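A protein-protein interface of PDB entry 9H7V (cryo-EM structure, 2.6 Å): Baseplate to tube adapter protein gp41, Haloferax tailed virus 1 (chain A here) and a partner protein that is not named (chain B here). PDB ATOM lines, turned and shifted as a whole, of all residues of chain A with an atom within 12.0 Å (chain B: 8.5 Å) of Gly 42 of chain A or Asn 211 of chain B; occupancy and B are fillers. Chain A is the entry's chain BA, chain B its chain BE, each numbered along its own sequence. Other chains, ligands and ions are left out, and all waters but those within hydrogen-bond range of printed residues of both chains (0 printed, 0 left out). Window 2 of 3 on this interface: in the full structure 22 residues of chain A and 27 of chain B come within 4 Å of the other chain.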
ATOM      1  N   VAL A  37     -34.981 -35.558  23.093  1.00  0.00           N
ATOM      2  CA  VAL A  37     -34.431 -35.078  24.348  1.00  0.00           C
ATOM      3  C   VAL A  37     -33.104 -34.410  24.000  1.00  0.00           C
ATOM      4  O   VAL A  37     -32.253 -35.040  23.372  1.00  0.00           O
ATOM      5  CB  VAL A  37     -34.238 -36.248  25.334  1.00  0.00           C
ATOM      6  CG1 VAL A  37     -33.686 -35.799  26.676  1.00  0.00           C
ATOM      7  CG2 VAL A  37     -35.511 -37.057  25.528  1.00  0.00           C
ATOM      8  N   ARG A  38     -32.943 -33.138  24.385  1.00  0.00           N
ATOM      9  CA  ARG A  38     -31.768 -32.378  23.984  1.00  0.00           C
ATOM     10  C   ARG A  38     -30.535 -32.933  24.694  1.00  0.00           C
ATOM     11  O   ARG A  38     -30.584 -33.220  25.889  1.00  0.00           O
ATOM     12  CB  ARG A  38     -31.944 -30.876  24.234  1.00  0.00           C
ATOM     13  CG  ARG A  38     -33.183 -30.251  23.605  1.00  0.00           C
ATOM     14  CD  ARG A  38     -33.480 -30.618  22.162  1.00  0.00           C
ATOM     15  NE  ARG A  38     -34.704 -29.974  21.708  1.00  0.00           N
ATOM     16  CZ  ARG A  38     -35.183 -30.018  20.469  1.00  0.00           C
ATOM     17  NH1 ARG A  38     -36.304 -29.380  20.180  1.00  0.00           N
ATOM     18  NH2 ARG A  38     -34.544 -30.681  19.520  1.00  0.00           N
ATOM     19  N   LYS A  39     -29.444 -33.087  23.933  1.00  0.00           N
ATOM     20  CA  LYS A  39     -28.183 -33.587  24.461  1.00  0.00           C
ATOM     21  C   LYS A  39     -27.500 -32.524  25.318  1.00  0.00           C
ATOM     22  O   LYS A  39     -26.768 -32.863  26.245  1.00  0.00           O
ATOM     23  CB  LYS A  39     -27.259 -34.070  23.339  1.00  0.00           C
ATOM     24  CG  LYS A  39     -27.010 -35.573  23.304  1.00  0.00           C
ATOM     25  CD  LYS A  39     -28.083 -36.373  22.590  1.00  0.00           C
ATOM     26  CE  LYS A  39     -27.949 -36.334  21.082  1.00  0.00           C
ATOM     27  NZ  LYS A  39     -28.987 -37.156  20.418  1.00  0.00           N
ATOM     28  N   SER A  40     -27.749 -31.247  24.997  1.00  0.00           N
ATOM     29  CA  SER A  40     -27.135 -30.133  25.702  1.00  0.00           C
ATOM     30  C   SER A  40     -28.126 -28.981  25.876  1.00  0.00           C
ATOM     31  O   SER A  40     -29.332 -29.174  25.732  1.00  0.00           O
ATOM     32  CB  SER A  40     -25.877 -29.698  25.013  1.00  0.00           C
ATOM     33  OG  SER A  40     -25.105 -28.872  25.868  1.00  0.00           O
ATOM     34  N   GLY A  41     -27.597 -27.792  26.196  1.00  0.00           N
ATOM     35  CA  GLY A  41     -28.370 -26.652  26.662  1.00  0.00           C
ATOM     36  C   GLY A  41     -27.904 -26.221  28.050  1.00  0.00           C
ATOM     37  O   GLY A  41     -27.257 -27.001  28.744  1.00  0.00           O
ATOM     38  N   GLY A  42     -28.252 -24.994  28.456  1.00  0.00           N
ATOM     39  CA  GLY A  42     -27.714 -24.404  29.674  1.00  0.00           C
ATOM     40  C   GLY A  42     -28.523 -24.727  30.930  1.00  0.00           C
ATOM     41  O   GLY A  42     -28.350 -24.066  31.952  1.00  0.00           O
ATOM     42  N   SER A  43     -29.389 -25.744  30.847  1.00  0.00           N
ATOM     43  CA  SER A  43     -30.214 -26.189  31.962  1.00  0.00           C
ATOM     44  C   SER A  43     -29.544 -27.366  32.666  1.00  0.00           C
ATOM     45  O   SER A  43     -28.602 -27.945  32.131  1.00  0.00           O
ATOM     46  CB  SER A  43     -31.595 -26.561  31.487  1.00  0.00           C
ATOM     47  OG  SER A  43     -32.175 -25.516  30.724  1.00  0.00           O
ATOM     48  N   LEU A  44     -30.030 -27.708  33.867  1.00  0.00           N
ATOM     49  CA  LEU A  44     -29.621 -28.938  34.530  1.00  0.00           C
ATOM     50  C   LEU A  44     -30.304 -30.126  33.857  1.00  0.00           C
ATOM     51  O   LEU A  44     -29.689 -31.174  33.675  1.00  0.00           O
ATOM     52  CB  LEU A  44     -29.965 -28.877  36.022  1.00  0.00           C
ATOM     53  CG  LEU A  44     -28.907 -28.253  36.934  1.00  0.00           C
ATOM     54  CD1 LEU A  44     -29.509 -27.883  38.279  1.00  0.00           C
ATOM     55  CD2 LEU A  44     -27.718 -29.184  37.128  1.00  0.00           C
ATOM     56  N   ASN A  45     -31.574 -29.932  33.484  1.00  0.00           N
ATOM     57  CA  ASN A  45     -32.408 -30.980  32.920  1.00  0.00           C
ATOM     58  C   ASN A  45     -32.774 -30.606  31.485  1.00  0.00           C
ATOM     59  O   ASN A  45     -33.024 -29.436  31.205  1.00  0.00           O
ATOM     60  CB  ASN A  45     -33.649 -31.218  33.783  1.00  0.00           C
ATOM     61  CG  ASN A  45     -33.343 -31.384  35.257  1.00  0.00           C
ATOM     62  OD1 ASN A  45     -32.646 -32.314  35.654  1.00  0.00           O
ATOM     63  ND2 ASN A  45     -33.871 -30.491  36.079  1.00  0.00           N
ATOM     64  N   PRO A  46     -32.828 -31.573  30.537  1.00  0.00           N
ATOM     65  CA  PRO A  46     -33.060 -31.253  29.129  1.00  0.00           C
ATOM     66  C   PRO A  46     -34.483 -30.788  28.832  1.00  0.00           C
ATOM     67  O   PRO A  46     -35.429 -31.184  29.511  1.00  0.00           O
ATOM     68  CB  PRO A  46     -32.800 -32.587  28.417  1.00  0.00           C
ATOM     69  CG  PRO A  46     -33.140 -33.630  29.458  1.00  0.00           C
ATOM     70  CD  PRO A  46     -32.675 -33.020  30.762  1.00  0.00           C
ATOM     71  N   ARG A  47     -34.602 -29.929  27.816  1.00  0.00           N
ATOM     72  CA  ARG A  47     -35.874 -29.677  27.162  1.00  0.00           C
ATOM     73  C   ARG A  47     -36.188 -30.870  26.264  1.00  0.00           C
ATOM     74  O   ARG A  47     -35.281 -31.525  25.756  1.00  0.00           O
ATOM     75  CB  ARG A  47     -35.826 -28.371  26.365  1.00  0.00           C
ATOM     76  CG  ARG A  47     -35.843 -27.116  27.226  1.00  0.00           C
ATOM     77  CD  ARG A  47     -35.979 -25.851  26.404  1.00  0.00           C
ATOM     78  NE  ARG A  47     -35.948 -24.647  27.226  1.00  0.00           N
ATOM     79  CZ  ARG A  47     -37.009 -24.051  27.763  1.00  0.00           C
ATOM     80  NH1 ARG A  47     -36.849 -22.961  28.491  1.00  0.00           N
ATOM     81  NH2 ARG A  47     -38.223 -24.541  27.577  1.00  0.00           N
ATOM     82  N   VAL A  48     -37.486 -31.152  26.099  1.00  0.00           N
ATOM     83  CA  VAL A  48     -37.949 -32.302  25.335  1.00  0.00           C
ATOM     84  C   VAL A  48     -39.036 -31.861  24.356  1.00  0.00           C
ATOM     85  O   VAL A  48     -39.617 -30.788  24.510  1.00  0.00           O
ATOM     86  CB  VAL A  48     -38.431 -33.456  26.240  1.00  0.00           C
ATOM     87  CG1 VAL A  48     -37.293 -34.094  27.022  1.00  0.00           C
ATOM     88  CG2 VAL A  48     -39.571 -33.052  27.165  1.00  0.00           C
ATOM     89  N   GLY B 208     -36.551 -14.566  21.934  1.00  0.00           N
ATOM     90  CA  GLY B 208     -35.116 -14.639  22.155  1.00  0.00           C
ATOM     91  C   GLY B 208     -34.638 -16.081  22.298  1.00  0.00           C
ATOM     92  O   GLY B 208     -35.437 -17.015  22.256  1.00  0.00           O
ATOM     93  N   VAL B 209     -33.319 -16.243  22.443  1.00  0.00           N
ATOM     94  CA  VAL B 209     -32.720 -17.530  22.750  1.00  0.00           C
ATOM     95  C   VAL B 209     -31.947 -17.366  24.057  1.00  0.00           C
ATOM     96  O   VAL B 209     -30.775 -16.993  24.048  1.00  0.00           O
ATOM     97  CB  VAL B 209     -31.826 -18.051  21.602  1.00  0.00           C
ATOM     98  CG1 VAL B 209     -31.321 -19.463  21.863  1.00  0.00           C
ATOM     99  CG2 VAL B 209     -32.516 -17.991  20.246  1.00  0.00           C
ATOM    100  N   ASP B 210     -32.635 -17.614  25.180  1.00  0.00           N
ATOM    101  CA  ASP B 210     -31.993 -17.586  26.484  1.00  0.00           C
ATOM    102  C   ASP B 210     -31.168 -18.859  26.662  1.00  0.00           C
ATOM    103  O   ASP B 210     -31.211 -19.757  25.821  1.00  0.00           O
ATOM    104  CB  ASP B 210     -32.981 -17.271  27.615  1.00  0.00           C
ATOM    105  CG  ASP B 210     -33.890 -18.417  28.029  1.00  0.00           C
ATOM    106  OD1 ASP B 210     -33.369 -19.453  28.479  1.00  0.00           O
ATOM    107  OD2 ASP B 210     -35.119 -18.250  27.925  1.00  0.00           O
ATOM    108  N   ASN B 211     -30.446 -18.926  27.788  1.00  0.00           N
ATOM    109  CA  ASN B 211     -29.450 -19.949  28.067  1.00  0.00           C
ATOM    110  C   ASN B 211     -30.077 -21.343  28.137  1.00  0.00           C
ATOM    111  O   ASN B 211     -29.377 -22.336  27.952  1.00  0.00           O
ATOM    112  CB  ASN B 211     -28.644 -19.597  29.321  1.00  0.00           C
ATOM    113  CG  ASN B 211     -27.346 -20.365  29.457  1.00  0.00           C
ATOM    114  OD1 ASN B 211     -26.561 -20.455  28.517  1.00  0.00           O
ATOM    115  ND2 ASN B 211     -27.100 -20.904  30.639  1.00  0.00           N
ATOM    116  N   THR B 212     -31.394 -21.417  28.377  1.00  0.00           N
ATOM    117  CA  THR B 212     -32.083 -22.693  28.517  1.00  0.00           C
ATOM    118  C   THR B 212     -32.552 -23.237  27.165  1.00  0.00           C
ATOM    119  O   THR B 212     -32.896 -24.416  27.079  1.00  0.00           O
ATOM    120  CB  THR B 212     -33.252 -22.623  29.512  1.00  0.00           C
ATOM    121  OG1 THR B 212     -34.301 -21.832  28.951  1.00  0.00           O
ATOM    122  CG2 THR B 212     -32.861 -22.086  30.871  1.00  0.00           C
ATOM    123  N   GLN B 213     -32.562 -22.397  26.115  1.00  0.00           N
ATOM    124  CA  GLN B 213     -33.266 -22.760  24.889  1.00  0.00           C
ATOM    125  C   GLN B 213     -32.379 -22.858  23.639  1.00  0.00           C
ATOM    126  O   GLN B 213     -32.896 -23.150  22.563  1.00  0.00           O
ATOM    127  CB  GLN B 213     -34.617 -22.044  24.719  1.00  0.00           C
ATOM    128  CG  GLN B 213     -34.671 -20.562  25.071  1.00  0.00           C
ATOM    129  CD  GLN B 213     -36.086 -20.028  25.062  1.00  0.00           C
ATOM    130  OE1 GLN B 213     -37.034 -20.701  24.658  1.00  0.00           O
ATOM    131  NE2 GLN B 213     -36.245 -18.794  25.512  1.00  0.00           N
ATOM    132  N   TRP B 214     -31.061 -22.645  23.770  1.00  0.00           N
ATOM    133  CA  TRP B 214     -30.109 -23.160  22.790  1.00  0.00           C
ATOM    134  C   TRP B 214     -29.771 -24.596  23.188  1.00  0.00           C
ATOM    135  O   TRP B 214     -29.952 -24.950  24.351  1.00  0.00           O
ATOM    136  CB  TRP B 214     -28.842 -22.291  22.715  1.00  0.00           C
ATOM    137  CG  TRP B 214     -28.025 -22.352  23.970  1.00  0.00           C
ATOM    138  CD1 TRP B 214     -28.116 -21.504  25.033  1.00  0.00           C
ATOM    139  CD2 TRP B 214     -27.037 -23.338  24.326  1.00  0.00           C
ATOM    140  NE1 TRP B 214     -27.245 -21.880  26.017  1.00  0.00           N
ATOM    141  CE2 TRP B 214     -26.575 -23.005  25.618  1.00  0.00           C
ATOM    142  CE3 TRP B 214     -26.489 -24.460  23.688  1.00  0.00           C
ATOM    143  CZ2 TRP B 214     -25.596 -23.749  26.276  1.00  0.00           C
ATOM    144  CZ3 TRP B 214     -25.531 -25.205  24.343  1.00  0.00           C
ATOM    145  CH2 TRP B 214     -25.087 -24.848  25.618  1.00  0.00           C
ATOM    146  N   PHE B 215     -29.267 -25.412  22.246  1.00  0.00           N
ATOM    147  CA  PHE B 215     -28.766 -26.739  22.597  1.00  0.00           C
ATOM    148  C   PHE B 215     -27.620 -27.213  21.697  1.00  0.00           C
ATOM    149  O   PHE B 215     -27.100 -28.309  21.899  1.00  0.00           O
ATOM    150  CB  PHE B 215     -29.889 -27.769  22.771  1.00  0.00           C
ATOM    151  CG  PHE B 215     -30.926 -27.793  21.680  1.00  0.00           C
ATOM    152  CD1 PHE B 215     -30.726 -28.554  20.538  1.00  0.00           C
ATOM    153  CD2 PHE B 215     -32.104 -27.067  21.802  1.00  0.00           C
ATOM    154  CE1 PHE B 215     -31.681 -28.583  19.533  1.00  0.00           C
ATOM    155  CE2 PHE B 215     -33.056 -27.093  20.793  1.00  0.00           C
ATOM    156  CZ  PHE B 215     -32.838 -27.846  19.659  1.00  0.00           C
ATOM    157  N   ARG B 216     -27.229 -26.385  20.720  1.00  0.00           N
ATOM    158  CA  ARG B 216     -26.006 -26.556  19.948  1.00  0.00           C
ATOM    159  C   ARG B 216     -25.595 -25.182  19.426  1.00  0.00           C
ATOM    160  O   ARG B 216     -26.453 -24.331  19.193  1.00  0.00           O
ATOM    161  CB  ARG B 216     -26.221 -27.541  18.793  1.00  0.00           C
ATOM    162  CG  ARG B 216     -24.948 -28.065  18.141  1.00  0.00           C
ATOM    163  CD  ARG B 216     -25.205 -28.772  16.821  1.00  0.00           C
ATOM    164  NE  ARG B 216     -26.172 -29.852  16.971  1.00  0.00           N
ATOM    165  CZ  ARG B 216     -27.286 -30.009  16.259  1.00  0.00           C
ATOM    166  NH1 ARG B 216     -28.079 -31.034  16.515  1.00  0.00           N
ATOM    167  NH2 ARG B 216     -27.596 -29.166  15.288  1.00  0.00           N
ATOM    168  N   TYR B 217     -24.284 -24.975  19.257  1.00  0.00           N
ATOM    169  CA  TYR B 217     -23.769 -23.754  18.657  1.00  0.00           C
ATOM    170  C   TYR B 217     -22.482 -24.058  17.892  1.00  0.00           C
ATOM    171  O   TYR B 217     -21.810 -25.049  18.169  1.00  0.00           O
ATOM    172  CB  TYR B 217     -23.595 -22.662  19.717  1.00  0.00           C
ATOM    173  CG  TYR B 217     -22.424 -22.890  20.636  1.00  0.00           C
ATOM    174  CD1 TYR B 217     -21.145 -22.522  20.251  1.00  0.00           C
ATOM    175  CD2 TYR B 217     -22.588 -23.497  21.874  1.00  0.00           C
ATOM    176  CE1 TYR B 217     -20.054 -22.747  21.071  1.00  0.00           C
ATOM    177  CE2 TYR B 217     -21.506 -23.723  22.711  1.00  0.00           C
ATOM    178  CZ  TYR B 217     -20.238 -23.345  22.304  1.00  0.00           C
ATOM    179  OH  TYR B 217     -19.157 -23.550  23.107  1.00  0.00           O
ATOM    180  N   ASP B 313     -32.380 -11.590  20.482  1.00  0.00           N
ATOM    181  CA  ASP B 313     -31.499 -11.694  21.636  1.00  0.00           C
ATOM    182  C   ASP B 313     -31.023 -13.139  21.767  1.00  0.00           C
ATOM    183  O   ASP B 313     -31.838 -14.059  21.758  1.00  0.00           O
ATOM    184  CB  ASP B 313     -32.214 -11.287  22.930  1.00  0.00           C
ATOM    185  CG  ASP B 313     -32.312  -9.792  23.195  1.00  0.00           C
ATOM    186  OD1 ASP B 313     -31.533  -9.024  22.595  1.00  0.00           O
ATOM    187  OD2 ASP B 313     -33.169  -9.406  24.016  1.00  0.00           O
ATOM    188  N   ILE B 314     -29.700 -13.330  21.880  1.00  0.00           N
ATOM    189  CA  ILE B 314     -29.122 -14.648  22.106  1.00  0.00           C
ATOM    190  C   ILE B 314     -28.215 -14.596  23.334  1.00  0.00           C
ATOM    191  O   ILE B 314     -27.324 -13.751  23.416  1.00  0.00           O
ATOM    192  CB  ILE B 314     -28.391 -15.189  20.855  1.00  0.00           C
ATOM    193  CG1 ILE B 314     -29.322 -15.281  19.642  1.00  0.00           C
ATOM    194  CG2 ILE B 314     -27.724 -16.529  21.152  1.00  0.00           C
ATOM    195  CD1 ILE B 314     -28.679 -15.821  18.383  1.00  0.00           C
ATOM    196  N   THR B 315     -28.467 -15.514  24.277  1.00  0.00           N
ATOM    197  CA  THR B 315     -27.626 -15.741  25.441  1.00  0.00           C
ATOM    198  C   THR B 315     -27.117 -17.180  25.407  1.00  0.00           C
ATOM    199  O   THR B 315     -27.909 -18.120  25.461  1.00  0.00           O
ATOM    200  CB  THR B 315     -28.387 -15.472  26.747  1.00  0.00           C
ATOM    201  OG1 THR B 315     -29.053 -14.211  26.666  1.00  0.00           O
ATOM    202  CG2 THR B 315     -27.500 -15.493  27.974  1.00  0.00           C
ATOM    203  N   ILE B 316     -25.792 -17.336  25.288  1.00  0.00           N
ATOM    204  CA  ILE B 316     -25.128 -18.622  25.441  1.00  0.00           C
ATOM    205  C   ILE B 316     -23.979 -18.433  26.428  1.00  0.00           C
ATOM    206  O   ILE B 316     -22.902 -17.971  26.050  1.00  0.00           O
ATOM    207  CB  ILE B 316     -24.659 -19.209  24.088  1.00  0.00           C
ATOM    208  CG1 ILE B 316     -25.766 -19.215  23.028  1.00  0.00           C
ATOM    209  CG2 ILE B 316     -24.078 -20.605  24.284  1.00  0.00           C
ATOM    210  CD1 ILE B 316     -25.279 -19.432  21.611  1.00  0.00           C
ATOM    211  N   ASP B 317     -24.236 -18.783  27.695  1.00  0.00           N
ATOM    212  CA  ASP B 317     -23.316 -18.548  28.800  1.00  0.00           C
ATOM    213  C   ASP B 317     -22.012 -19.330  28.627  1.00  0.00           C
ATOM    214  O   ASP B 317     -20.947 -18.751  28.834  1.00  0.00           O
ATOM    215  CB  ASP B 317     -23.983 -18.767  30.162  1.00  0.00           C
ATOM    216  CG  ASP B 317     -24.954 -17.671  30.576  1.00  0.00           C
ATOM    217  OD1 ASP B 317     -24.927 -16.585  29.957  1.00  0.00           O
ATOM    218  OD2 ASP B 317     -25.730 -17.911  31.523  1.00  0.00           O
ATOM    219  N   PRO B 318     -22.025 -20.642  28.271  1.00  0.00           N
ATOM    220  CA  PRO B 318     -20.783 -21.383  28.025  1.00  0.00           C
ATOM    221  C   PRO B 318     -19.889 -20.831  26.915  1.00  0.00           C
ATOM    222  O   PRO B 318     -18.718 -21.197  26.826  1.00  0.00           O
ATOM    223  CB  PRO B 318     -21.278 -22.784  27.637  1.00  0.00           C
ATOM    224  CG  PRO B 318     -22.619 -22.895  28.318  1.00  0.00           C
ATOM    225  CD  PRO B 318     -23.210 -21.513  28.158  1.00  0.00           C
ATOM    226  N   ARG B 319     -20.450 -19.932  26.093  1.00  0.00           N
ATOM    227  CA  ARG B 319     -19.786 -19.364  24.929  1.00  0.00           C
ATOM    228  C   ARG B 319     -19.484 -17.879  25.155  1.00  0.00           C
ATOM    229  O   ARG B 319     -18.730 -17.272  24.394  1.00  0.00           O
ATOM    230  CB  ARG B 319     -20.623 -19.673  23.678  1.00  0.00           C
ATOM    231  CG  ARG B 319     -20.091 -19.146  22.353  1.00  0.00           C
ATOM    232  CD  ARG B 319     -18.673 -19.544  21.990  1.00  0.00           C
ATOM    233  NE  ARG B 319     -18.214 -18.879  20.778  1.00  0.00           N
ATOM    234  CZ  ARG B 319     -17.777 -17.624  20.700  1.00  0.00           C
ATOM    235  NH1 ARG B 319     -17.396 -17.142  19.531  1.00  0.00           N
ATOM    236  NH2 ARG B 319     -17.734 -16.849  21.771  1.00  0.00           N
ATOM    237  N   GLY B 320     -20.064 -17.306  26.218  1.00  0.00           N
ATOM    238  CA  GLY B 320     -19.819 -15.926  26.611  1.00  0.00           C
ATOM    239  C   GLY B 320     -20.572 -14.919  25.745  1.00  0.00           C
ATOM    240  O   GLY B 320     -20.157 -13.767  25.635  1.00  0.00           O
ATOM    241  N   ILE B 321     -21.689 -15.367  25.156  1.00  0.00           N
ATOM    242  CA  ILE B 321     -22.483 -14.578  24.226  1.00  0.00           C
ATOM    243  C   ILE B 321     -23.740 -14.082  24.940  1.00  0.00           C
ATOM    244  O   ILE B 321     -24.444 -14.865  25.574  1.00  0.00           O
ATOM    245  CB  ILE B 321     -22.794 -15.396  22.951  1.00  0.00           C
ATOM    246  CG1 ILE B 321     -21.575 -15.467  22.025  1.00  0.00           C
ATOM    247  CG2 ILE B 321     -24.028 -14.868  22.224  1.00  0.00           C
ATOM    248  CD1 ILE B 321     -21.751 -16.346  20.803  1.00  0.00           C
ATOM    249  N   ASP B 322     -23.992 -12.769  24.830  1.00  0.00           N
ATOM    250  CA  ASP B 322     -25.189 -12.131  25.358  1.00  0.00           C
ATOM    251  C   ASP B 322     -25.479 -10.876  24.534  1.00  0.00           C
ATOM    252  O   ASP B 322     -25.254  -9.757  24.996  1.00  0.00           O
ATOM    253  CB  ASP B 322     -25.063 -11.866  26.863  1.00  0.00           C
ATOM    254  CG  ASP B 322     -26.377 -11.532  27.550  1.00  0.00           C
ATOM    255  OD1 ASP B 322     -27.418 -12.100  27.154  1.00  0.00           O
ATOM    256  OD2 ASP B 322     -26.349 -10.708  28.486  1.00  0.00           O
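Among the printed residues, pairs that only touch across the chains: Gly 41 of chain A with Trp 214 of chain B (3.3 Å), Arg 38 of chain A with Phe 215 of chain B (3.3 Å), Ser 43 of chain A with Thr 212 of chain B (3.3 Å), Ser 40 of chain A with Phe 215 of chain B (3.3 Å), Gly 42 of chain A with Trp 214 of chain B (3.7 Å), Arg 47 of chain A with Gln 213 of chain B (3.9 Å), Gly 41 of chain A with Phe 215 of chain B (3.9 Å) and Ser 40 of chain A with Trp 214 of chain B (3.99 Å).
Of the 20 printed residues of chain B, 5 touch a printed residue of chain A.
Printed residues of chain B that touch a printed residue of chain A: Asn 211, Thr 212, Gln 213, Trp 214 and Phe 215.
Hydrophobic or aromatic side chains of chain B within 4 Å of the printed part of chain A: Trp 214 and Phe 215.
Printed residues of chain A that touch a printed residue of chain B: Arg 38, Ser 40, Gly 41, Gly 42, Ser 43 and Arg 47.
Among the printed residues, no Asp or Glu carboxylate lies within 4 Å of a Lys or Arg side-chain nitrogen of the other chain.
N of Arg 38 of chain A sits at hydrogen-bond distance from O of Arg 47 of chain A, at 3.2 Å.
The side-chain carboxylate of Asp 210 of chain B lies within hydrogen-bond range of the side-chain hydroxyl of Thr 212 of chain B (2.6 Å).
O of Asn 211 of chain B is in hydrogen-bond range of NE1 of Trp 214 of chain B, at 2.9 Å.
NE2 of Gln 213 of chain B is in hydrogen-bond range of OD2 of Asp 210 of chain B, at 2.7 Å.
The side-chain amide oxygen (OD1) of Asn 211 of chain B is in hydrogen-bond range of the backbone NH (N) of Asp 317 of chain B (3.0 Å).
The guanidinium group of Arg 47 of chain A lies within hydrogen-bond range of the side-chain hydroxyl of Thr 212 of chain B (2.8 Å).
The backbone carbonyl oxygen of Asn 211 of chain B lies within hydrogen-bond range of the backbone NH of Gly 42 of chain A.
Gly 41 of chain A touches two residues of chain B.
Gly 42 of chain A touches just these residues of chain B: Asn 211 (2.9 Å) and Trp 214 (3.7 Å).
Pro 46 of chain A touches none of the printed residues of chain B.
Printed residues of chain B within 4 Å of Arg 47 of chain A: Thr 212 and Gln 213.
Gly 208 of chain B touches none of the printed residues of chain A.
No residue of chain A comes within 4 Å of Asp 210 of chain B.
Printed residues of chain A within 4 Å of Asn 211 of chain B: Gly 42.
Of chain A, only Ser 43 and Arg 47 come within 4 Å of Thr 212 of chain B.
Of chain A, only Arg 47 (3.9 Å) comes within 4 Å of Gln 213 of chain B.
Printed residues of chain A within 4 Å of Trp 214 of chain B: Ser 40 (3.99 Å), Gly 41 (3.3 Å) and Gly 42 (3.7 Å).
Of the printed residues of chain A, Phe 215 of chain B touches Arg 38 (3.3 Å), Ser 40 (3.3 Å) and Gly 41 (3.9 Å).
No residue of chain A comes within 4 Å of Thr 315 of chain B.
The nearest residue of chain B that does not touch Gly 42 of chain A is Thr 212 of chain B (4.5 Å).
The nearest residue of chain A that does not touch Asn 211 of chain B is Gly 41 of chain A (4.2 Å).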
